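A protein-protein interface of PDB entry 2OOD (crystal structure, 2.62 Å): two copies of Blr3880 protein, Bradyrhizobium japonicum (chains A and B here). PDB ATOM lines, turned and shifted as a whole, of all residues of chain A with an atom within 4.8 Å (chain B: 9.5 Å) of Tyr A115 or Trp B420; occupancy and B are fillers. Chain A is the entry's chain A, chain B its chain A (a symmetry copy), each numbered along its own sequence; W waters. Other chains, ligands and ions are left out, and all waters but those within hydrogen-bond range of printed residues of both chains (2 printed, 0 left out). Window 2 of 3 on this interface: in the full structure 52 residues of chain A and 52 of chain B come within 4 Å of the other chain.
Water W1 bridges O of Thr A85 (2.7 Å) and O of Ala B417 (2.7 Å). Water W2 lies within hydrogen-bond range of the indole nitrogen of Trp B420 (2.9 Å) and the side-chain carboxylate of Glu A118 (3.1 Å).
The side-chain hydroxyl (OH) of Tyr A115 is in hydrogen-bond range of the guanidinium group (NH1) of Arg A86, 2.9 Å away. The side-chain amino group of Lys A109 lies within salt-bridge range of the side-chain carboxylate of Glu A106, 3.0 Å away. The backbone NH (N) of Tyr A115 lies within hydrogen-bond range of the side-chain carboxylate (OD2) of Asp A112. The guanidinium group (NE) of Arg A122 is in salt-bridge range of the side-chain carboxylate (OE2) of Glu A118, at 2.5 Å. The backbone carbonyl oxygen (O) of Trp B420 sits at hydrogen-bond distance from the side-chain hydroxyl (OG) of Ser B423, 2.9 Å away. O of Ser B423 lies within hydrogen-bond range of N of Gly B428 (3.2 Å).
Hydrophobic or aromatic side chains of chain A that line the printed part of chain B: Tyr A115. Of the 18 printed residues of chain B, 4 touch a printed residue of chain A. Hydrophobic or aromatic side chains of chain B within 4 Å of the printed part of chain A: Trp B420, His B421 and Leu B424. Among the printed residues, 8 pairs touch across the chains.
The backbone carbonyl oxygen of Trp B420 sits at hydrogen-bond distance from the guanidinium group of Arg A86 (2.7 Å). The guanidinium group (NH2) of Arg A86 lies within hydrogen-bond range of the side-chain hydroxyl (OG) of Ser B423.
Printed residues of chain B within 4 Å of Arg A86: Trp B420, His B421, Ser B423 and Leu B424. No residue of chain B comes within 4 Å of Asn A114. Tyr A115 touches one residue of chain B. No residue of chain B comes within 4 Å of Ala A116. No residue of chain B comes within 4 Å of Glu A118. Of the printed residues of chain B, Gly A119 touches Trp B420 (3.99 Å). Gly B413 touches none of the printed residues of chain A. Of the printed residues of chain A, Trp B420 touches Arg A86, Tyr A115, Gly A119 and Arg A122. Of the printed residues of chain A, His B421 touches Arg A86 (2.8 Å). Of the printed residues of chain A, Ser B423 touches Arg A86. Of the printed residues of chain A, Leu B424 touches Arg A86 (3.3 Å) and Lys A109 (3.8 Å). The nearest printed residue of chain A that does not touch Trp B420 is Tyr A110 (4.01 Å). The nearest printed residue of chain B that does not touch Gly A119 is Ala B417 (9.4 Å).
Among the printed residues, merely in contact across the chains: Arg A86 with His B421, Arg A86 with Leu B424, Arg A122 with Trp B420, Lys A109 with Leu B424, Tyr A115 with Trp B420 and Gly A119 with Trp B420.
No position is printed for both chains. Of the 8 pairs that touch across the chains among the printed residues, none has its exchanged pair printed and touching as well.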
ATOM      1  N   THR A  85      -3.008 -10.699 -29.223  1.00  0.00           N
ATOM      2  CA  THR A  85      -3.113 -11.696 -28.162  1.00  0.00           C
ATOM      3  C   THR A  85      -3.092 -11.124 -26.748  1.00  0.00           C
ATOM      4  O   THR A  85      -3.752 -11.643 -25.852  1.00  0.00           O
ATOM      5  CB  THR A  85      -1.954 -12.718 -28.261  1.00  0.00           C
ATOM      6  OG1 THR A  85      -2.049 -13.435 -29.496  1.00  0.00           O
ATOM      7  CG2 THR A  85      -1.989 -13.694 -27.099  1.00  0.00           C
ATOM      8  N   ARG A  86      -2.337 -10.052 -26.551  1.00  0.00           N
ATOM      9  CA  ARG A  86      -2.194  -9.462 -25.230  1.00  0.00           C
ATOM     10  C   ARG A  86      -3.119  -8.299 -24.917  1.00  0.00           C
ATOM     11  O   ARG A  86      -3.181  -7.857 -23.768  1.00  0.00           O
ATOM     12  CB  ARG A  86      -0.745  -9.019 -25.044  1.00  0.00           C
ATOM     13  CG  ARG A  86      -0.354  -8.689 -23.622  1.00  0.00           C
ATOM     14  CD  ARG A  86       1.119  -8.358 -23.548  1.00  0.00           C
ATOM     15  NE  ARG A  86       1.573  -8.263 -22.168  1.00  0.00           N
ATOM     16  CZ  ARG A  86       2.819  -7.972 -21.806  1.00  0.00           C
ATOM     17  NH1 ARG A  86       3.740  -7.742 -22.732  1.00  0.00           N
ATOM     18  NH2 ARG A  86       3.142  -7.920 -20.517  1.00  0.00           N
ATOM     19  N   GLU A 106       0.553  -1.786 -29.768  1.00  0.00           N
ATOM     20  CA  GLU A 106       0.938  -3.135 -29.333  1.00  0.00           C
ATOM     21  C   GLU A 106       1.483  -3.970 -30.483  1.00  0.00           C
ATOM     22  O   GLU A 106       2.475  -4.673 -30.330  1.00  0.00           O
ATOM     23  CB  GLU A 106      -0.269  -3.851 -28.717  1.00  0.00           C
ATOM     24  CG  GLU A 106      -0.094  -5.345 -28.447  1.00  0.00           C
ATOM     25  CD  GLU A 106       0.868  -5.654 -27.310  1.00  0.00           C
ATOM     26  OE1 GLU A 106       1.085  -4.772 -26.446  1.00  0.00           O
ATOM     27  OE2 GLU A 106       1.393  -6.793 -27.273  1.00  0.00           O
ATOM     28  N   LYS A 109       5.171  -3.776 -31.529  1.00  0.00           N
ATOM     29  CA  LYS A 109       6.182  -4.481 -30.734  1.00  0.00           C
ATOM     30  C   LYS A 109       6.657  -5.760 -31.422  1.00  0.00           C
ATOM     31  O   LYS A 109       7.759  -6.243 -31.159  1.00  0.00           O
ATOM     32  CB  LYS A 109       5.630  -4.870 -29.360  1.00  0.00           C
ATOM     33  CG  LYS A 109       5.100  -3.738 -28.517  1.00  0.00           C
ATOM     34  CD  LYS A 109       4.581  -4.296 -27.199  1.00  0.00           C
ATOM     35  CE  LYS A 109       4.032  -3.216 -26.289  1.00  0.00           C
ATOM     36  NZ  LYS A 109       3.537  -3.792 -25.009  1.00  0.00           N
ATOM     37  N   TYR A 110       5.818  -6.314 -32.289  1.00  0.00           N
ATOM     38  CA  TYR A 110       6.169  -7.538 -32.986  1.00  0.00           C
ATOM     39  C   TYR A 110       7.256  -7.355 -34.037  1.00  0.00           C
ATOM     40  O   TYR A 110       7.588  -8.295 -34.763  1.00  0.00           O
ATOM     41  CB  TYR A 110       4.916  -8.175 -33.598  1.00  0.00           C
ATOM     42  CG  TYR A 110       4.032  -8.816 -32.550  1.00  0.00           C
ATOM     43  CD1 TYR A 110       3.383  -8.047 -31.591  1.00  0.00           C
ATOM     44  CD2 TYR A 110       3.894 -10.193 -32.476  1.00  0.00           C
ATOM     45  CE1 TYR A 110       2.625  -8.635 -30.585  1.00  0.00           C
ATOM     46  CE2 TYR A 110       3.140 -10.791 -31.475  1.00  0.00           C
ATOM     47  CZ  TYR A 110       2.510 -10.009 -30.533  1.00  0.00           C
ATOM     48  OH  TYR A 110       1.770 -10.604 -29.530  1.00  0.00           O
ATOM     49  N   ASP A 112      10.149  -6.581 -33.138  1.00  0.00           N
ATOM     50  CA  ASP A 112      11.190  -7.237 -32.356  1.00  0.00           C
ATOM     51  C   ASP A 112      10.919  -8.744 -32.399  1.00  0.00           C
ATOM     52  O   ASP A 112       9.850  -9.195 -31.979  1.00  0.00           O
ATOM     53  CB  ASP A 112      11.116  -6.715 -30.924  1.00  0.00           C
ATOM     54  CG  ASP A 112      12.116  -7.369 -30.013  1.00  0.00           C
ATOM     55  OD1 ASP A 112      13.022  -6.658 -29.523  1.00  0.00           O
ATOM     56  OD2 ASP A 112      11.997  -8.594 -29.783  1.00  0.00           O
ATOM     57  N   ARG A 113      11.880  -9.523 -32.893  1.00  0.00           N
ATOM     58  CA  ARG A 113      11.683 -10.964 -33.023  1.00  0.00           C
ATOM     59  C   ARG A 113      11.510 -11.743 -31.724  1.00  0.00           C
ATOM     60  O   ARG A 113      10.869 -12.796 -31.718  1.00  0.00           O
ATOM     61  CB  ARG A 113      12.811 -11.579 -33.842  1.00  0.00           C
ATOM     62  CG  ARG A 113      12.545 -13.010 -34.236  1.00  0.00           C
ATOM     63  CD  ARG A 113      13.699 -13.554 -35.041  1.00  0.00           C
ATOM     64  NE  ARG A 113      13.892 -12.833 -36.299  1.00  0.00           N
ATOM     65  CZ  ARG A 113      13.060 -12.889 -37.336  1.00  0.00           C
ATOM     66  NH1 ARG A 113      11.961 -13.633 -37.280  1.00  0.00           N
ATOM     67  NH2 ARG A 113      13.339 -12.216 -38.443  1.00  0.00           N
ATOM     68  N   ASN A 114      12.069 -11.246 -30.627  1.00  0.00           N
ATOM     69  CA  ASN A 114      11.920 -11.936 -29.351  1.00  0.00           C
ATOM     70  C   ASN A 114      10.485 -11.842 -28.857  1.00  0.00           C
ATOM     71  O   ASN A 114       9.903 -12.835 -28.411  1.00  0.00           O
ATOM     72  CB  ASN A 114      12.867 -11.351 -28.302  1.00  0.00           C
ATOM     73  CG  ASN A 114      14.310 -11.742 -28.545  1.00  0.00           C
ATOM     74  OD1 ASN A 114      14.669 -12.922 -28.482  1.00  0.00           O
ATOM     75  ND2 ASN A 114      15.147 -10.753 -28.837  1.00  0.00           N
ATOM     76  N   TYR A 115       9.917 -10.642 -28.939  1.00  0.00           N
ATOM     77  CA  TYR A 115       8.539 -10.407 -28.518  1.00  0.00           C
ATOM     78  C   TYR A 115       7.609 -11.198 -29.431  1.00  0.00           C
ATOM     79  O   TYR A 115       6.665 -11.824 -28.975  1.00  0.00           O
ATOM     80  CB  TYR A 115       8.203  -8.921 -28.622  1.00  0.00           C
ATOM     81  CG  TYR A 115       6.999  -8.500 -27.826  1.00  0.00           C
ATOM     82  CD1 TYR A 115       7.108  -8.190 -26.483  1.00  0.00           C
ATOM     83  CD2 TYR A 115       5.749  -8.404 -28.415  1.00  0.00           C
ATOM     84  CE1 TYR A 115       6.003  -7.788 -25.741  1.00  0.00           C
ATOM     85  CE2 TYR A 115       4.631  -8.004 -27.682  1.00  0.00           C
ATOM     86  CZ  TYR A 115       4.768  -7.694 -26.343  1.00  0.00           C
ATOM     87  OH  TYR A 115       3.675  -7.267 -25.604  1.00  0.00           O
ATOM     88  N   ALA A 116       7.886 -11.158 -30.727  1.00  0.00           N
ATOM     89  CA  ALA A 116       7.076 -11.867 -31.701  1.00  0.00           C
ATOM     90  C   ALA A 116       7.068 -13.353 -31.392  1.00  0.00           C
ATOM     91  O   ALA A 116       6.022 -14.006 -31.442  1.00  0.00           O
ATOM     92  CB  ALA A 116       7.615 -11.630 -33.105  1.00  0.00           C
ATOM     93  N   ARG A 117       8.243 -13.891 -31.076  1.00  0.00           N
ATOM     94  CA  ARG A 117       8.361 -15.313 -30.769  1.00  0.00           C
ATOM     95  C   ARG A 117       7.549 -15.692 -29.530  1.00  0.00           C
ATOM     96  O   ARG A 117       6.929 -16.756 -29.487  1.00  0.00           O
ATOM     97  CB  ARG A 117       9.829 -15.697 -30.570  1.00  0.00           C
ATOM     98  CG  ARG A 117      10.021 -17.179 -30.319  1.00  0.00           C
ATOM     99  CD  ARG A 117      11.459 -17.519 -29.969  1.00  0.00           C
ATOM    100  NE  ARG A 117      12.365 -17.261 -31.080  1.00  0.00           N
ATOM    101  CZ  ARG A 117      13.354 -16.373 -31.047  1.00  0.00           C
ATOM    102  NH1 ARG A 117      13.560 -15.649 -29.948  1.00  0.00           N
ATOM    103  NH2 ARG A 117      14.148 -16.219 -32.103  1.00  0.00           N
ATOM    104  N   GLU A 118       7.546 -14.821 -28.525  1.00  0.00           N
ATOM    105  CA  GLU A 118       6.794 -15.098 -27.308  1.00  0.00           C
ATOM    106  C   GLU A 118       5.287 -14.988 -27.541  1.00  0.00           C
ATOM    107  O   GLU A 118       4.516 -15.805 -27.035  1.00  0.00           O
ATOM    108  CB  GLU A 118       7.200 -14.143 -26.198  1.00  0.00           C
ATOM    109  CG  GLU A 118       7.244 -14.827 -24.855  1.00  0.00           C
ATOM    110  CD  GLU A 118       6.769 -13.930 -23.732  1.00  0.00           C
ATOM    111  OE1 GLU A 118       7.188 -12.742 -23.691  1.00  0.00           O
ATOM    112  OE2 GLU A 118       5.980 -14.425 -22.886  1.00  0.00           O
ATOM    113  N   GLY A 119       4.871 -13.973 -28.299  1.00  0.00           N
ATOM    114  CA  GLY A 119       3.461 -13.799 -28.591  1.00  0.00           C
ATOM    115  C   GLY A 119       2.950 -15.001 -29.359  1.00  0.00           C
ATOM    116  O   GLY A 119       1.916 -15.569 -29.017  1.00  0.00           O
ATOM    117  N   ARG A 122       2.346 -17.838 -27.003  1.00  0.00           N
ATOM    118  CA  ARG A 122       1.147 -17.659 -26.189  1.00  0.00           C
ATOM    119  C   ARG A 122      -0.123 -17.696 -27.030  1.00  0.00           C
ATOM    120  O   ARG A 122      -1.168 -18.166 -26.575  1.00  0.00           O
ATOM    121  CB  ARG A 122       1.234 -16.340 -25.431  1.00  0.00           C
ATOM    122  CG  ARG A 122       2.295 -16.346 -24.362  1.00  0.00           C
ATOM    123  CD  ARG A 122       2.620 -14.949 -23.936  1.00  0.00           C
ATOM    124  NE  ARG A 122       3.556 -14.924 -22.819  1.00  0.00           N
ATOM    125  CZ  ARG A 122       3.279 -15.366 -21.594  1.00  0.00           C
ATOM    126  NH1 ARG A 122       2.084 -15.877 -21.318  1.00  0.00           N
ATOM    127  NH2 ARG A 122       4.198 -15.283 -20.639  1.00  0.00           N
ATOM    128  N   PRO B 411      -7.375 -11.402 -10.190  1.00  0.00           N
ATOM    129  CA  PRO B 411      -7.288 -10.786 -11.519  1.00  0.00           C
ATOM    130  C   PRO B 411      -6.671 -11.645 -12.617  1.00  0.00           C
ATOM    131  O   PRO B 411      -6.828 -11.344 -13.794  1.00  0.00           O
ATOM    132  CB  PRO B 411      -6.509  -9.494 -11.257  1.00  0.00           C
ATOM    133  CG  PRO B 411      -5.711  -9.805 -10.031  1.00  0.00           C
ATOM    134  CD  PRO B 411      -6.671 -10.588  -9.185  1.00  0.00           C
ATOM    135  N   ASN B 412      -5.989 -12.722 -12.240  1.00  0.00           N
ATOM    136  CA  ASN B 412      -5.361 -13.589 -13.230  1.00  0.00           C
ATOM    137  C   ASN B 412      -6.221 -14.768 -13.657  1.00  0.00           C
ATOM    138  O   ASN B 412      -5.841 -15.525 -14.548  1.00  0.00           O
ATOM    139  CB  ASN B 412      -4.012 -14.102 -12.717  1.00  0.00           C
ATOM    140  CG  ASN B 412      -2.917 -13.055 -12.812  1.00  0.00           C
ATOM    141  OD1 ASN B 412      -2.686 -12.485 -13.878  1.00  0.00           O
ATOM    142  ND2 ASN B 412      -2.232 -12.802 -11.699  1.00  0.00           N
ATOM    143  N   GLY B 413      -7.382 -14.913 -13.031  1.00  0.00           N
ATOM    144  CA  GLY B 413      -8.265 -16.016 -13.364  1.00  0.00           C
ATOM    145  C   GLY B 413      -8.997 -15.852 -14.679  1.00  0.00           C
ATOM    146  O   GLY B 413      -9.260 -14.733 -15.119  1.00  0.00           O
ATOM    147  N   GLY B 414      -9.332 -16.973 -15.309  1.00  0.00           N
ATOM    148  CA  GLY B 414     -10.037 -16.921 -16.573  1.00  0.00           C
ATOM    149  C   GLY B 414      -9.287 -17.662 -17.654  1.00  0.00           C
ATOM    150  O   GLY B 414      -8.411 -18.466 -17.360  1.00  0.00           O
ATOM    151  N   GLN B 415      -9.629 -17.394 -18.909  1.00  0.00           N
ATOM    152  CA  GLN B 415      -8.976 -18.047 -20.037  1.00  0.00           C
ATOM    153  C   GLN B 415      -7.459 -17.868 -19.961  1.00  0.00           C
ATOM    154  O   GLN B 415      -6.959 -16.984 -19.262  1.00  0.00           O
ATOM    155  CB  GLN B 415      -9.514 -17.477 -21.355  1.00  0.00           C
ATOM    156  CG  GLN B 415      -9.233 -15.996 -21.551  1.00  0.00           C
ATOM    157  CD  GLN B 415      -9.908 -15.426 -22.775  1.00  0.00           C
ATOM    158  OE1 GLN B 415      -9.803 -15.974 -23.864  1.00  0.00           O
ATOM    159  NE2 GLN B 415     -10.602 -14.311 -22.601  1.00  0.00           N
ATOM    160  N   LEU B 416      -6.739 -18.712 -20.693  1.00  0.00           N
ATOM    161  CA  LEU B 416      -5.281 -18.698 -20.729  1.00  0.00           C
ATOM    162  C   LEU B 416      -4.638 -17.333 -20.965  1.00  0.00           C
ATOM    163  O   LEU B 416      -3.585 -17.038 -20.403  1.00  0.00           O
ATOM    164  CB  LEU B 416      -4.784 -19.656 -21.815  1.00  0.00           C
ATOM    165  CG  LEU B 416      -3.785 -20.753 -21.447  1.00  0.00           C
ATOM    166  CD1 LEU B 416      -3.041 -21.188 -22.698  1.00  0.00           C
ATOM    167  CD2 LEU B 416      -2.807 -20.235 -20.412  1.00  0.00           C
ATOM    168  N   ALA B 417      -5.266 -16.510 -21.801  1.00  0.00           N
ATOM    169  CA  ALA B 417      -4.735 -15.192 -22.149  1.00  0.00           C
ATOM    170  C   ALA B 417      -4.724 -14.131 -21.057  1.00  0.00           C
ATOM    171  O   ALA B 417      -4.005 -13.140 -21.170  1.00  0.00           O
ATOM    172  CB  ALA B 417      -5.478 -14.653 -23.362  1.00  0.00           C
ATOM    173  N   GLN B 418      -5.514 -14.329 -20.008  1.00  0.00           N
ATOM    174  CA  GLN B 418      -5.609 -13.356 -18.919  1.00  0.00           C
ATOM    175  C   GLN B 418      -4.357 -12.779 -18.288  1.00  0.00           C
ATOM    176  O   GLN B 418      -4.147 -11.567 -18.308  1.00  0.00           O
ATOM    177  CB  GLN B 418      -6.459 -13.900 -17.774  1.00  0.00           C
ATOM    178  CG  GLN B 418      -7.851 -13.341 -17.684  1.00  0.00           C
ATOM    179  CD  GLN B 418      -7.901 -11.871 -17.308  1.00  0.00           C
ATOM    180  OE1 GLN B 418      -7.208 -11.032 -17.889  1.00  0.00           O
ATOM    181  NE2 GLN B 418      -8.747 -11.551 -16.341  1.00  0.00           N
ATOM    182  N   PRO B 419      -3.512 -13.639 -17.698  1.00  0.00           N
ATOM    183  CA  PRO B 419      -2.301 -13.157 -17.051  1.00  0.00           C
ATOM    184  C   PRO B 419      -1.253 -12.424 -17.863  1.00  0.00           C
ATOM    185  O   PRO B 419      -0.527 -11.639 -17.285  1.00  0.00           O
ATOM    186  CB  PRO B 419      -1.762 -14.415 -16.368  1.00  0.00           C
ATOM    187  CG  PRO B 419      -2.124 -15.533 -17.343  1.00  0.00           C
ATOM    188  CD  PRO B 419      -3.505 -15.115 -17.789  1.00  0.00           C
ATOM    189  N   TRP B 420      -1.145 -12.668 -19.170  1.00  0.00           N
ATOM    190  CA  TRP B 420      -0.154 -11.937 -19.967  1.00  0.00           C
ATOM    191  C   TRP B 420      -0.761 -10.604 -20.318  1.00  0.00           C
ATOM    192  O   TRP B 420      -0.058  -9.627 -20.575  1.00  0.00           O
ATOM    193  CB  TRP B 420       0.237 -12.687 -21.239  1.00  0.00           C
ATOM    194  CG  TRP B 420       1.465 -12.095 -21.851  1.00  0.00           C
ATOM    195  CD1 TRP B 420       2.579 -11.679 -21.188  1.00  0.00           C
ATOM    196  CD2 TRP B 420       1.713 -11.849 -23.240  1.00  0.00           C
ATOM    197  NE1 TRP B 420       3.504 -11.185 -22.070  1.00  0.00           N
ATOM    198  CE2 TRP B 420       2.999 -11.278 -23.338  1.00  0.00           C
ATOM    199  CE3 TRP B 420       0.977 -12.054 -24.412  1.00  0.00           C
ATOM    200  CZ2 TRP B 420       3.564 -10.912 -24.562  1.00  0.00           C
ATOM    201  CZ3 TRP B 420       1.546 -11.689 -25.632  1.00  0.00           C
ATOM    202  CH2 TRP B 420       2.825 -11.125 -25.693  1.00  0.00           C
ATOM    203  N   HIS B 421      -2.089 -10.581 -20.326  1.00  0.00           N
ATOM    204  CA  HIS B 421      -2.850  -9.376 -20.615  1.00  0.00           C
ATOM    205  C   HIS B 421      -2.820  -8.443 -19.406  1.00  0.00           C
ATOM    206  O   HIS B 421      -2.596  -7.234 -19.523  1.00  0.00           O
ATOM    207  CB  HIS B 421      -4.296  -9.744 -20.955  1.00  0.00           C
ATOM    208  CG  HIS B 421      -5.215  -8.564 -21.015  1.00  0.00           C
ATOM    209  ND1 HIS B 421      -6.260  -8.388 -20.132  1.00  0.00           N
ATOM    210  CD2 HIS B 421      -5.219  -7.478 -21.822  1.00  0.00           C
ATOM    211  CE1 HIS B 421      -6.866  -7.243 -20.390  1.00  0.00           C
ATOM    212  NE2 HIS B 421      -6.253  -6.672 -21.411  1.00  0.00           N
ATOM    213  N   GLN B 422      -3.059  -9.024 -18.239  1.00  0.00           N
ATOM    214  CA  GLN B 422      -3.066  -8.274 -16.994  1.00  0.00           C
ATOM    215  C   GLN B 422      -1.670  -7.756 -16.640  1.00  0.00           C
ATOM    216  O   GLN B 422      -1.542  -6.710 -15.999  1.00  0.00           O
ATOM    217  CB  GLN B 422      -3.603  -9.159 -15.864  1.00  0.00           C
ATOM    218  CG  GLN B 422      -5.089  -9.460 -15.963  1.00  0.00           C
ATOM    219  CD  GLN B 422      -5.953  -8.341 -15.406  1.00  0.00           C
ATOM    220  OE1 GLN B 422      -5.650  -7.161 -15.579  1.00  0.00           O
ATOM    221  NE2 GLN B 422      -7.043  -8.708 -14.748  1.00  0.00           N
ATOM    222  N   SER B 423      -0.628  -8.471 -17.063  1.00  0.00           N
ATOM    223  CA  SER B 423       0.742  -8.059 -16.748  1.00  0.00           C
ATOM    224  C   SER B 423       1.155  -6.768 -17.448  1.00  0.00           C
ATOM    225  O   SER B 423       2.206  -6.200 -17.146  1.00  0.00           O
ATOM    226  CB  SER B 423       1.742  -9.163 -17.109  1.00  0.00           C
ATOM    227  OG  SER B 423       1.972  -9.224 -18.505  1.00  0.00           O
ATOM    228  N   LEU B 424       0.332  -6.307 -18.387  1.00  0.00           N
ATOM    229  CA  LEU B 424       0.624  -5.070 -19.110  1.00  0.00           C
ATOM    230  C   LEU B 424       0.516  -3.868 -18.186  1.00  0.00           C
ATOM    231  O   LEU B 424       0.978  -2.782 -18.520  1.00  0.00           O
ATOM    232  CB  LEU B 424      -0.347  -4.872 -20.276  1.00  0.00           C
ATOM    233  CG  LEU B 424       0.061  -5.409 -21.645  1.00  0.00           C
ATOM    234  CD1 LEU B 424      -1.050  -5.124 -22.642  1.00  0.00           C
ATOM    235  CD2 LEU B 424       1.364  -4.756 -22.099  1.00  0.00           C
ATOM    236  N   ILE B 425      -0.091  -4.061 -17.022  1.00  0.00           N
ATOM    237  CA  ILE B 425      -0.267  -2.964 -16.086  1.00  0.00           C
ATOM    238  C   ILE B 425       0.955  -2.656 -15.219  1.00  0.00           C
ATOM    239  O   ILE B 425       1.084  -3.137 -14.093  1.00  0.00           O
ATOM    240  CB  ILE B 425      -1.496  -3.221 -15.207  1.00  0.00           C
ATOM    241  CG1 ILE B 425      -2.731  -3.269 -16.104  1.00  0.00           C
ATOM    242  CG2 ILE B 425      -1.654  -2.121 -14.154  1.00  0.00           C
ATOM    243  CD1 ILE B 425      -4.006  -3.199 -15.355  1.00  0.00           C
ATOM    244  N   GLY B 428       3.889  -5.710 -14.476  1.00  0.00           N
ATOM    245  CA  GLY B 428       4.463  -6.674 -13.556  1.00  0.00           C
ATOM    246  C   GLY B 428       3.389  -7.459 -12.810  1.00  0.00           C
ATOM    247  O   GLY B 428       3.007  -8.555 -13.238  1.00  0.00           O
ATOM    248  N   ALA B 443     -10.515  -6.107 -16.911  1.00  0.00           N
ATOM    249  CA  ALA B 443     -10.019  -7.329 -17.519  1.00  0.00           C
ATOM    250  C   ALA B 443     -10.741  -8.520 -16.889  1.00  0.00           C
ATOM    251  O   ALA B 443     -10.920  -9.551 -17.530  1.00  0.00           O
ATOM    252  CB  ALA B 443      -8.526  -7.447 -17.314  1.00  0.00           C
ATOM    253  N   VAL B 447     -12.154 -10.210 -20.010  1.00  0.00           N
ATOM    254  CA  VAL B 447     -11.273 -11.306 -20.399  1.00  0.00           C
ATOM    255  C   VAL B 447     -11.424 -12.544 -19.527  1.00  0.00           C
ATOM    256  O   VAL B 447     -11.102 -13.650 -19.960  1.00  0.00           O
ATOM    257  CB  VAL B 447      -9.799 -10.871 -20.396  1.00  0.00           C
ATOM    258  CG1 VAL B 447      -8.941 -11.953 -21.002  1.00  0.00           C
ATOM    259  CG2 VAL B 447      -9.642  -9.592 -21.175  1.00  0.00           C
HETATM  260  O   HOH W   1      -2.832 -12.636 -23.568  1.00  0.00           O
HETATM  261  O   HOH W   2       6.299 -10.686 -21.595  1.00  0.00           O
